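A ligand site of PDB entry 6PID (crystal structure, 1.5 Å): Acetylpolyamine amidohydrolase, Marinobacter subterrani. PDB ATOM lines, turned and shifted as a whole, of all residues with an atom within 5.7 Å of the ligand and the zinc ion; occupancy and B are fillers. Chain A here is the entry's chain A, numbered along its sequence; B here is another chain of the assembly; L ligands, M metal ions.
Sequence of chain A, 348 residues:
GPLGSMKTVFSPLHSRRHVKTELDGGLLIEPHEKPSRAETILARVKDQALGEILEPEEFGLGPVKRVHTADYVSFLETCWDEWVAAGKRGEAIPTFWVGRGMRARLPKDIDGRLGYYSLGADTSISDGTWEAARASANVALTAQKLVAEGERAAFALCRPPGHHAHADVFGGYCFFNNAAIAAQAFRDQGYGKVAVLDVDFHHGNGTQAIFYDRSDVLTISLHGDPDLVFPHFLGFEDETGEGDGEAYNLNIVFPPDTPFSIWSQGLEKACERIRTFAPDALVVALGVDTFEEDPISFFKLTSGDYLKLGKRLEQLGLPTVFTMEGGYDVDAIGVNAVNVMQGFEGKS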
ATOM      1  N   GLU A  22      -2.958  28.505  22.984  1.00  0.00           N
ATOM      2  CA  GLU A  22      -3.165  27.595  21.867  1.00  0.00           C
ATOM      3  C   GLU A  22      -4.166  28.223  20.918  1.00  0.00           C
ATOM      4  O   GLU A  22      -5.265  28.592  21.340  1.00  0.00           O
ATOM      5  CB  GLU A  22      -3.681  26.216  22.325  1.00  0.00           C
ATOM      6  CG  GLU A  22      -4.032  25.264  21.165  1.00  0.00           C
ATOM      7  CD  GLU A  22      -4.505  23.893  21.639  1.00  0.00           C
ATOM      8  OE1 GLU A  22      -4.310  23.561  22.822  1.00  0.00           O
ATOM      9  OE2 GLU A  22      -5.096  23.142  20.817  1.00  0.00           O
ATOM     10  N   LEU A  23      -3.787  28.376  19.654  1.00  0.00           N
ATOM     11  CA  LEU A  23      -4.740  28.834  18.660  1.00  0.00           C
ATOM     12  C   LEU A  23      -5.778  27.735  18.419  1.00  0.00           C
ATOM     13  O   LEU A  23      -5.422  26.589  18.130  1.00  0.00           O
ATOM     14  CB  LEU A  23      -4.035  29.194  17.355  1.00  0.00           C
ATOM     15  CG  LEU A  23      -4.952  29.606  16.193  1.00  0.00           C
ATOM     16  CD1 LEU A  23      -5.682  30.922  16.469  1.00  0.00           C
ATOM     17  CD2 LEU A  23      -4.204  29.678  14.860  1.00  0.00           C
ATOM     18  N   ASP A  24      -7.046  28.083  18.581  1.00  0.00           N
ATOM     19  CA  ASP A  24      -8.142  27.126  18.416  1.00  0.00           C
ATOM     20  C   ASP A  24      -9.403  27.895  18.061  1.00  0.00           C
ATOM     21  O   ASP A  24      -9.909  28.682  18.875  1.00  0.00           O
ATOM     22  CB  ASP A  24      -8.318  26.302  19.680  1.00  0.00           C
ATOM     23  CG  ASP A  24      -9.275  25.165  19.490  1.00  0.00           C
ATOM     24  OD1 ASP A  24      -8.946  24.234  18.736  1.00  0.00           O
ATOM     25  OD2 ASP A  24     -10.363  25.198  20.090  1.00  0.00           O
ATOM     26  N   GLY A  25      -9.910  27.690  16.853  1.00  0.00           N
ATOM     27  CA  GLY A  25     -11.173  28.289  16.459  1.00  0.00           C
ATOM     28  C   GLY A  25     -11.149  29.794  16.426  1.00  0.00           C
ATOM     29  O   GLY A  25     -12.128  30.449  16.829  1.00  0.00           O
ATOM     30  N   ILE A  29      -6.633  30.048  23.272  1.00  0.00           N
ATOM     31  CA  ILE A  29      -7.283  29.370  24.381  1.00  0.00           C
ATOM     32  C   ILE A  29      -6.230  28.742  25.288  1.00  0.00           C
ATOM     33  O   ILE A  29      -5.036  28.732  24.982  1.00  0.00           O
ATOM     34  CB  ILE A  29      -8.290  28.313  23.891  1.00  0.00           C
ATOM     35  CG1 ILE A  29      -7.564  27.034  23.489  1.00  0.00           C
ATOM     36  CG2 ILE A  29      -9.091  28.842  22.706  1.00  0.00           C
ATOM     37  CD1 ILE A  29      -8.504  25.867  23.261  1.00  0.00           C
ATOM     38  N   HIS A  32      -4.596  22.354  25.553  1.00  0.00           N
ATOM     39  CA  HIS A  32      -5.074  21.037  25.940  1.00  0.00           C
ATOM     40  C   HIS A  32      -3.952  20.164  26.475  1.00  0.00           C
ATOM     41  O   HIS A  32      -4.154  19.385  27.402  1.00  0.00           O
ATOM     42  CB  HIS A  32      -5.715  20.330  24.755  1.00  0.00           C
ATOM     43  CG  HIS A  32      -6.961  20.977  24.233  1.00  0.00           C
ATOM     44  ND1 HIS A  32      -8.199  20.817  24.826  1.00  0.00           N
ATOM     45  CD2 HIS A  32      -7.170  21.773  23.151  1.00  0.00           C
ATOM     46  CE1 HIS A  32      -9.110  21.495  24.151  1.00  0.00           C
ATOM     47  NE2 HIS A  32      -8.507  22.085  23.130  1.00  0.00           N
ATOM     48  N   ASP A 122      -1.206  25.605  16.286  1.00  0.00           N
ATOM     49  CA  ASP A 122      -1.756  25.332  17.607  1.00  0.00           C
ATOM     50  C   ASP A 122      -0.708  24.815  18.586  1.00  0.00           C
ATOM     51  O   ASP A 122      -1.059  24.394  19.685  1.00  0.00           O
ATOM     52  CB  ASP A 122      -2.917  24.344  17.507  1.00  0.00           C
ATOM     53  CG  ASP A 122      -2.528  23.068  16.785  1.00  0.00           C
ATOM     54  OD1 ASP A 122      -1.381  22.971  16.329  1.00  0.00           O
ATOM     55  OD2 ASP A 122      -3.382  22.166  16.681  1.00  0.00           O
ATOM     56  N   HIS A 163       3.934  11.794  17.809  1.00  0.00           N
ATOM     57  CA  HIS A 163       3.635  11.054  16.586  1.00  0.00           C
ATOM     58  C   HIS A 163       3.282  11.934  15.392  1.00  0.00           C
ATOM     59  O   HIS A 163       3.238  11.432  14.257  1.00  0.00           O
ATOM     60  CB  HIS A 163       2.542   9.996  16.834  1.00  0.00           C
ATOM     61  CG  HIS A 163       1.179  10.524  17.137  1.00  0.00           C
ATOM     62  ND1 HIS A 163       0.031   9.908  16.688  1.00  0.00           N
ATOM     63  CD2 HIS A 163       0.760  11.581  17.880  1.00  0.00           C
ATOM     64  CE1 HIS A 163      -1.030  10.574  17.115  1.00  0.00           C
ATOM     65  NE2 HIS A 163      -0.611  11.588  17.847  1.00  0.00           N
ATOM     66  N   HIS A 164       3.089  13.236  15.584  1.00  0.00           N
ATOM     67  CA  HIS A 164       2.819  14.095  14.443  1.00  0.00           C
ATOM     68  C   HIS A 164       4.064  14.707  13.830  1.00  0.00           C
ATOM     69  O   HIS A 164       3.996  15.224  12.715  1.00  0.00           O
ATOM     70  CB  HIS A 164       1.857  15.216  14.851  1.00  0.00           C
ATOM     71  CG  HIS A 164       0.482  14.731  15.180  1.00  0.00           C
ATOM     72  ND1 HIS A 164      -0.218  13.872  14.361  1.00  0.00           N
ATOM     73  CD2 HIS A 164      -0.335  14.995  16.225  1.00  0.00           C
ATOM     74  CE1 HIS A 164      -1.408  13.621  14.890  1.00  0.00           C
ATOM     75  NE2 HIS A 164      -1.503  14.304  16.015  1.00  0.00           N
ATOM     76  N   GLY A 172       0.772  19.579  15.978  1.00  0.00           N
ATOM     77  CA  GLY A 172      -0.086  18.694  16.751  1.00  0.00           C
ATOM     78  C   GLY A 172       0.478  18.377  18.124  1.00  0.00           C
ATOM     79  O   GLY A 172       0.322  17.253  18.611  1.00  0.00           O
ATOM     80  N   TYR A 173       1.164  19.337  18.738  1.00  0.00           N
ATOM     81  CA  TYR A 173       1.704  19.299  20.089  1.00  0.00           C
ATOM     82  C   TYR A 173       3.019  18.533  20.135  1.00  0.00           C
ATOM     83  O   TYR A 173       3.565  18.373  21.239  1.00  0.00           O
ATOM     84  CB  TYR A 173       0.720  18.690  21.106  1.00  0.00           C
ATOM     85  CG  TYR A 173      -0.716  19.233  21.045  1.00  0.00           C
ATOM     86  CD1 TYR A 173      -0.998  20.513  20.613  1.00  0.00           C
ATOM     87  CD2 TYR A 173      -1.787  18.426  21.448  1.00  0.00           C
ATOM     88  CE1 TYR A 173      -2.330  20.996  20.582  1.00  0.00           C
ATOM     89  CE2 TYR A 173      -3.079  18.879  21.418  1.00  0.00           C
ATOM     90  CZ  TYR A 173      -3.350  20.157  20.995  1.00  0.00           C
ATOM     91  OH  TYR A 173      -4.674  20.568  20.977  1.00  0.00           O
ATOM     92  N   CYS A 174       3.553  18.075  18.990  1.00  0.00           N
ATOM     93  CA  CYS A 174       4.718  17.189  18.930  1.00  0.00           C
ATOM     94  C   CYS A 174       5.929  17.888  18.331  1.00  0.00           C
ATOM     95  O   CYS A 174       5.796  18.641  17.362  1.00  0.00           O
ATOM     96  CB  CYS A 174       4.434  15.950  18.079  1.00  0.00           C
ATOM     97  SG  CYS A 174       2.986  15.037  18.595  1.00  0.00           S
ATOM     98  N   ASP A 200      -3.442   6.078  19.172  1.00  0.00           N
ATOM     99  CA  ASP A 200      -3.934   7.436  19.398  1.00  0.00           C
ATOM    100  C   ASP A 200      -5.097   7.723  18.454  1.00  0.00           C
ATOM    101  O   ASP A 200      -5.152   7.207  17.330  1.00  0.00           O
ATOM    102  CB  ASP A 200      -2.796   8.441  19.186  1.00  0.00           C
ATOM    103  CG  ASP A 200      -3.193   9.878  19.488  1.00  0.00           C
ATOM    104  OD1 ASP A 200      -3.851  10.514  18.623  1.00  0.00           O
ATOM    105  OD2 ASP A 200      -2.827  10.386  20.573  1.00  0.00           O
ATOM    106  N   PHE A 201      -6.044   8.555  18.916  1.00  0.00           N
ATOM    107  CA  PHE A 201      -7.192   8.917  18.094  1.00  0.00           C
ATOM    108  C   PHE A 201      -6.805   9.519  16.752  1.00  0.00           C
ATOM    109  O   PHE A 201      -7.573   9.415  15.778  1.00  0.00           O
ATOM    110  CB  PHE A 201      -8.109   9.919  18.824  1.00  0.00           C
ATOM    111  CG  PHE A 201      -9.177  10.528  17.934  1.00  0.00           C
ATOM    112  CD1 PHE A 201     -10.330   9.817  17.622  1.00  0.00           C
ATOM    113  CD2 PHE A 201      -8.997  11.793  17.363  1.00  0.00           C
ATOM    114  CE1 PHE A 201     -11.302  10.343  16.801  1.00  0.00           C
ATOM    115  CE2 PHE A 201      -9.969  12.334  16.522  1.00  0.00           C
ATOM    116  CZ  PHE A 201     -11.123  11.623  16.246  1.00  0.00           C
ATOM    117  N   HIS A 202      -5.665  10.207  16.675  1.00  0.00           N
ATOM    118  CA  HIS A 202      -5.259  10.906  15.466  1.00  0.00           C
ATOM    119  C   HIS A 202      -4.245  10.109  14.672  1.00  0.00           C
ATOM    120  O   HIS A 202      -3.483   9.295  15.224  1.00  0.00           O
ATOM    121  CB  HIS A 202      -4.638  12.272  15.788  1.00  0.00           C
ATOM    122  CG  HIS A 202      -5.547  13.202  16.530  1.00  0.00           C
ATOM    123  ND1 HIS A 202      -5.501  13.344  17.895  1.00  0.00           N
ATOM    124  CD2 HIS A 202      -6.529  14.016  16.095  1.00  0.00           C
ATOM    125  CE1 HIS A 202      -6.402  14.230  18.264  1.00  0.00           C
ATOM    126  NE2 HIS A 202      -7.043  14.645  17.189  1.00  0.00           N
ATOM    127  N   PHE A 230      -7.978  16.501  12.335  1.00  0.00           N
ATOM    128  CA  PHE A 230      -6.533  16.612  12.195  1.00  0.00           C
ATOM    129  C   PHE A 230      -5.910  15.219  12.107  1.00  0.00           C
ATOM    130  O   PHE A 230      -6.351  14.297  12.817  1.00  0.00           O
ATOM    131  CB  PHE A 230      -5.994  17.369  13.414  1.00  0.00           C
ATOM    132  CG  PHE A 230      -4.511  17.554  13.399  1.00  0.00           C
ATOM    133  CD1 PHE A 230      -3.952  18.650  12.755  1.00  0.00           C
ATOM    134  CD2 PHE A 230      -3.677  16.659  14.052  1.00  0.00           C
ATOM    135  CE1 PHE A 230      -2.582  18.838  12.743  1.00  0.00           C
ATOM    136  CE2 PHE A 230      -2.302  16.836  14.033  1.00  0.00           C
ATOM    137  CZ  PHE A 230      -1.759  17.927  13.385  1.00  0.00           C
ATOM    138  N   ASP A 289      -6.859   9.626  23.793  1.00  0.00           N
ATOM    139  CA  ASP A 289      -7.894  10.513  23.266  1.00  0.00           C
ATOM    140  C   ASP A 289      -8.933   9.772  22.426  1.00  0.00           C
ATOM    141  O   ASP A 289      -9.809  10.418  21.839  1.00  0.00           O
ATOM    142  CB  ASP A 289      -7.304  11.709  22.496  1.00  0.00           C
ATOM    143  CG  ASP A 289      -6.242  11.336  21.467  1.00  0.00           C
ATOM    144  OD1 ASP A 289      -5.957  10.150  21.226  1.00  0.00           O
ATOM    145  OD2 ASP A 289      -5.694  12.307  20.883  1.00  0.00           O
ATOM    146  N   ILE A 296     -11.480  16.738  22.316  1.00  0.00           N
ATOM    147  CA  ILE A 296     -11.253  17.129  20.933  1.00  0.00           C
ATOM    148  C   ILE A 296     -11.449  15.964  19.962  1.00  0.00           C
ATOM    149  O   ILE A 296     -11.110  16.087  18.789  1.00  0.00           O
ATOM    150  CB  ILE A 296      -9.858  17.765  20.766  1.00  0.00           C
ATOM    151  CG1 ILE A 296      -8.772  16.755  21.160  1.00  0.00           C
ATOM    152  CG2 ILE A 296      -9.767  19.047  21.593  1.00  0.00           C
ATOM    153  CD1 ILE A 296      -7.338  17.260  20.966  1.00  0.00           C
ATOM    154  N   SER A 297     -11.992  14.829  20.430  1.00  0.00           N
ATOM    155  CA  SER A 297     -12.024  13.609  19.642  1.00  0.00           C
ATOM    156  C   SER A 297     -13.418  12.999  19.676  1.00  0.00           C
ATOM    157  O   SER A 297     -14.247  13.351  20.522  1.00  0.00           O
ATOM    158  CB  SER A 297     -10.997  12.612  20.160  1.00  0.00           C
ATOM    159  OG  SER A 297      -9.765  13.260  20.453  1.00  0.00           O
ATOM    160  N   GLU A 325       1.216   9.471  23.910  1.00  0.00           N
ATOM    161  CA  GLU A 325       0.857  10.505  22.946  1.00  0.00           C
ATOM    162  C   GLU A 325      -0.270  11.370  23.493  1.00  0.00           C
ATOM    163  O   GLU A 325      -0.109  12.050  24.513  1.00  0.00           O
ATOM    164  CB  GLU A 325       0.470   9.872  21.602  1.00  0.00           C
ATOM    165  CG  GLU A 325       1.487   8.881  21.056  1.00  0.00           C
ATOM    166  CD  GLU A 325       2.794   9.518  20.622  1.00  0.00           C
ATOM    167  OE1 GLU A 325       2.810  10.737  20.387  1.00  0.00           O
ATOM    168  OE2 GLU A 325       3.800   8.800  20.518  1.00  0.00           O
ATOM    169  N   GLY A 326      -1.438  11.325  22.863  1.00  0.00           N
ATOM    170  CA  GLY A 326      -2.527  12.212  23.217  1.00  0.00           C
ATOM    171  C   GLY A 326      -3.378  11.685  24.367  1.00  0.00           C
ATOM    172  O   GLY A 326      -3.021  10.748  25.076  1.00  0.00           O
ATOM    173  N   GLY A 327      -4.528  12.352  24.564  1.00  0.00           N
ATOM    174  CA  GLY A 327      -5.437  12.091  25.663  1.00  0.00           C
ATOM    175  C   GLY A 327      -5.629  13.322  26.540  1.00  0.00           C
ATOM    176  O   GLY A 327      -4.686  13.733  27.224  1.00  0.00           O
ATOM    177  N   TYR A 328      -6.828  13.913  26.545  1.00  0.00           N
ATOM    178  CA  TYR A 328      -7.007  15.270  27.073  1.00  0.00           C
ATOM    179  C   TYR A 328      -8.150  15.421  28.072  1.00  0.00           C
ATOM    180  O   TYR A 328      -8.346  16.526  28.611  1.00  0.00           O
ATOM    181  CB  TYR A 328      -7.159  16.248  25.895  1.00  0.00           C
ATOM    182  CG  TYR A 328      -6.000  16.055  24.936  1.00  0.00           C
ATOM    183  CD1 TYR A 328      -4.723  16.517  25.253  1.00  0.00           C
ATOM    184  CD2 TYR A 328      -6.163  15.346  23.753  1.00  0.00           C
ATOM    185  CE1 TYR A 328      -3.658  16.323  24.402  1.00  0.00           C
ATOM    186  CE2 TYR A 328      -5.094  15.124  22.892  1.00  0.00           C
ATOM    187  CZ  TYR A 328      -3.845  15.633  23.218  1.00  0.00           C
ATOM    188  OH  TYR A 328      -2.786  15.432  22.373  1.00  0.00           O
ATOM    189  N   THR B  95      -5.826  26.922  11.391  1.00  0.00           N
ATOM    190  CA  THR B  95      -4.995  26.393  12.458  1.00  0.00           C
ATOM    191  C   THR B  95      -3.970  25.381  11.967  1.00  0.00           C
ATOM    192  O   THR B  95      -3.001  25.107  12.666  1.00  0.00           O
ATOM    193  CB  THR B  95      -5.870  25.732  13.534  1.00  0.00           C
ATOM    194  OG1 THR B  95      -7.018  26.568  13.770  1.00  0.00           O
ATOM    195  CG2 THR B  95      -5.097  25.535  14.849  1.00  0.00           C
ATOM    196  N   PHE B  96      -4.181  24.790  10.787  1.00  0.00           N
ATOM    197  CA  PHE B  96      -3.223  23.823  10.285  1.00  0.00           C
ATOM    198  C   PHE B  96      -3.389  23.730   8.771  1.00  0.00           C
ATOM    199  O   PHE B  96      -4.411  24.142   8.222  1.00  0.00           O
ATOM    200  CB  PHE B  96      -3.388  22.454  10.967  1.00  0.00           C
ATOM    201  CG  PHE B  96      -4.778  22.189  11.470  1.00  0.00           C
ATOM    202  CD1 PHE B  96      -5.034  22.070  12.837  1.00  0.00           C
ATOM    203  CD2 PHE B  96      -5.822  22.044  10.584  1.00  0.00           C
ATOM    204  CE1 PHE B  96      -6.321  21.821  13.293  1.00  0.00           C
ATOM    205  CE2 PHE B  96      -7.104  21.784  11.032  1.00  0.00           C
ATOM    206  CZ  PHE B  96      -7.358  21.684  12.388  1.00  0.00           C
HETATM  207  C1  LIG L   1      -6.322  22.878  17.529  1.00  0.00           C
HETATM  208  C2  LIG L   1      -6.806  21.459  18.008  1.00  0.00           C
HETATM  209  C3  LIG L   1      -6.529  20.344  16.930  1.00  0.00           C
HETATM  210  C4  LIG L   1      -6.144  18.945  17.520  1.00  0.00           C
HETATM  211  C5  LIG L   1      -4.631  18.555  17.362  1.00  0.00           C
HETATM  212  C6  LIG L   1      -4.325  17.026  17.502  1.00  0.00           C
HETATM  213  C7  LIG L   1      -3.394  16.684  18.705  1.00  0.00           C
HETATM  214  C8  LIG L   1      -3.300  15.226  19.147  1.00  0.00           C
HETATM  215  N1  LIG L   1      -6.235  23.911  18.659  1.00  0.00           N
HETATM  216  N2  LIG L   1      -2.526  14.291  18.505  1.00  0.00           N
HETATM  217  O1  LIG L   1      -2.503  12.975  19.029  1.00  0.00           O
HETATM  218  O2  LIG L   1      -3.991  14.900  20.177  1.00  0.00           O
HETATM  219 ZN    ZN M   1      -4.286  12.359  19.448  1.00  0.00          ZN
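The nearest printed residue that does not touch the zinc ion is His 163 (4.1 Å).
OD1 of Asp 289 is in hydrogen-bond range of N of Phe 201.
O of Asp 289 sits close to OG of Ser 297 (3.2 Å).
OD1 of Asp 200 lies close to NE2 of His 163, 3.5 Å away.
The side-chain carboxylate (OD2) of Asp 200 is in hydrogen-bond range of the backbone NH (N) of Gly 326 (2.8 Å).
The side-chain carboxylate (OE2) of Glu 22 is in hydrogen-bond range of the side-chain hydroxyl (OH) of Tyr 173.
OE1 of Glu 22 sits at hydrogen-bond distance from N of His 32.
The backbone NH of His 163 is in hydrogen-bond range of the side-chain carboxylate of Glu 325, at 3.0 Å.
The backbone NH (N) of His 164 lies within hydrogen-bond range of the side-chain sulfur (SG) of Cys 174, 3.5 Å away.
The side-chain carboxylate (OE2) of Glu 22 is in salt-bridge range of a nitrogen (N1) of the ligand (2.6 Å).
An oxygen (O2) of the ligand is in hydrogen-bond range of the side-chain hydroxyl of Tyr 328 (2.6 Å).
A nitrogen (N2) of the ligand is in hydrogen-bond range of a ring nitrogen (NE2) of His 163, 3.4 Å away.
A ring nitrogen (NE2) of His 164 is in hydrogen-bond range of a nitrogen (N2) of the ligand (2.7 Å).
A nitrogen (N1) of the ligand lies within salt-bridge range of the side-chain carboxylate (OD1) of Asp 24 (2.7 Å).
The backbone carbonyl oxygen (O) of Leu 23 is in hydrogen-bond range of a nitrogen (N1) of the ligand (2.8 Å).
OD2 of Asp 122 is in salt-bridge range of N1 of the ligand, at 3.9 Å.
Residues that only touch the ligand: Gly 172, Tyr 173, Phe 230, Thr 95 of chain B and Phe 96 of chain B.
Hydrophobic or aromatic side chains that line the ligand: His 163, His 164, Tyr 173, His 202, Phe 230, Tyr 328 and Phe 96 of chain B.
Of the 25 residues printed, 15 come within 4 Å of the ligand.
An oxygen (O1) of the ligand binds the zinc ion (1.9 Å).
The zinc ion is bound by OD2 of Asp 289 (2.0 Å).
The side-chain carboxylate (OD1) of Asp 200 is bound to the zinc ion, 2.1 Å away.
A ring nitrogen (ND1) of His 202 binds the zinc ion (2.2 Å).
Slightly farther from the zinc ion lies O2 of the ligand (2.7 Å).
Slightly farther from the zinc ion lies the side-chain carboxylate (OD2) of Asp 200 (2.7 Å).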
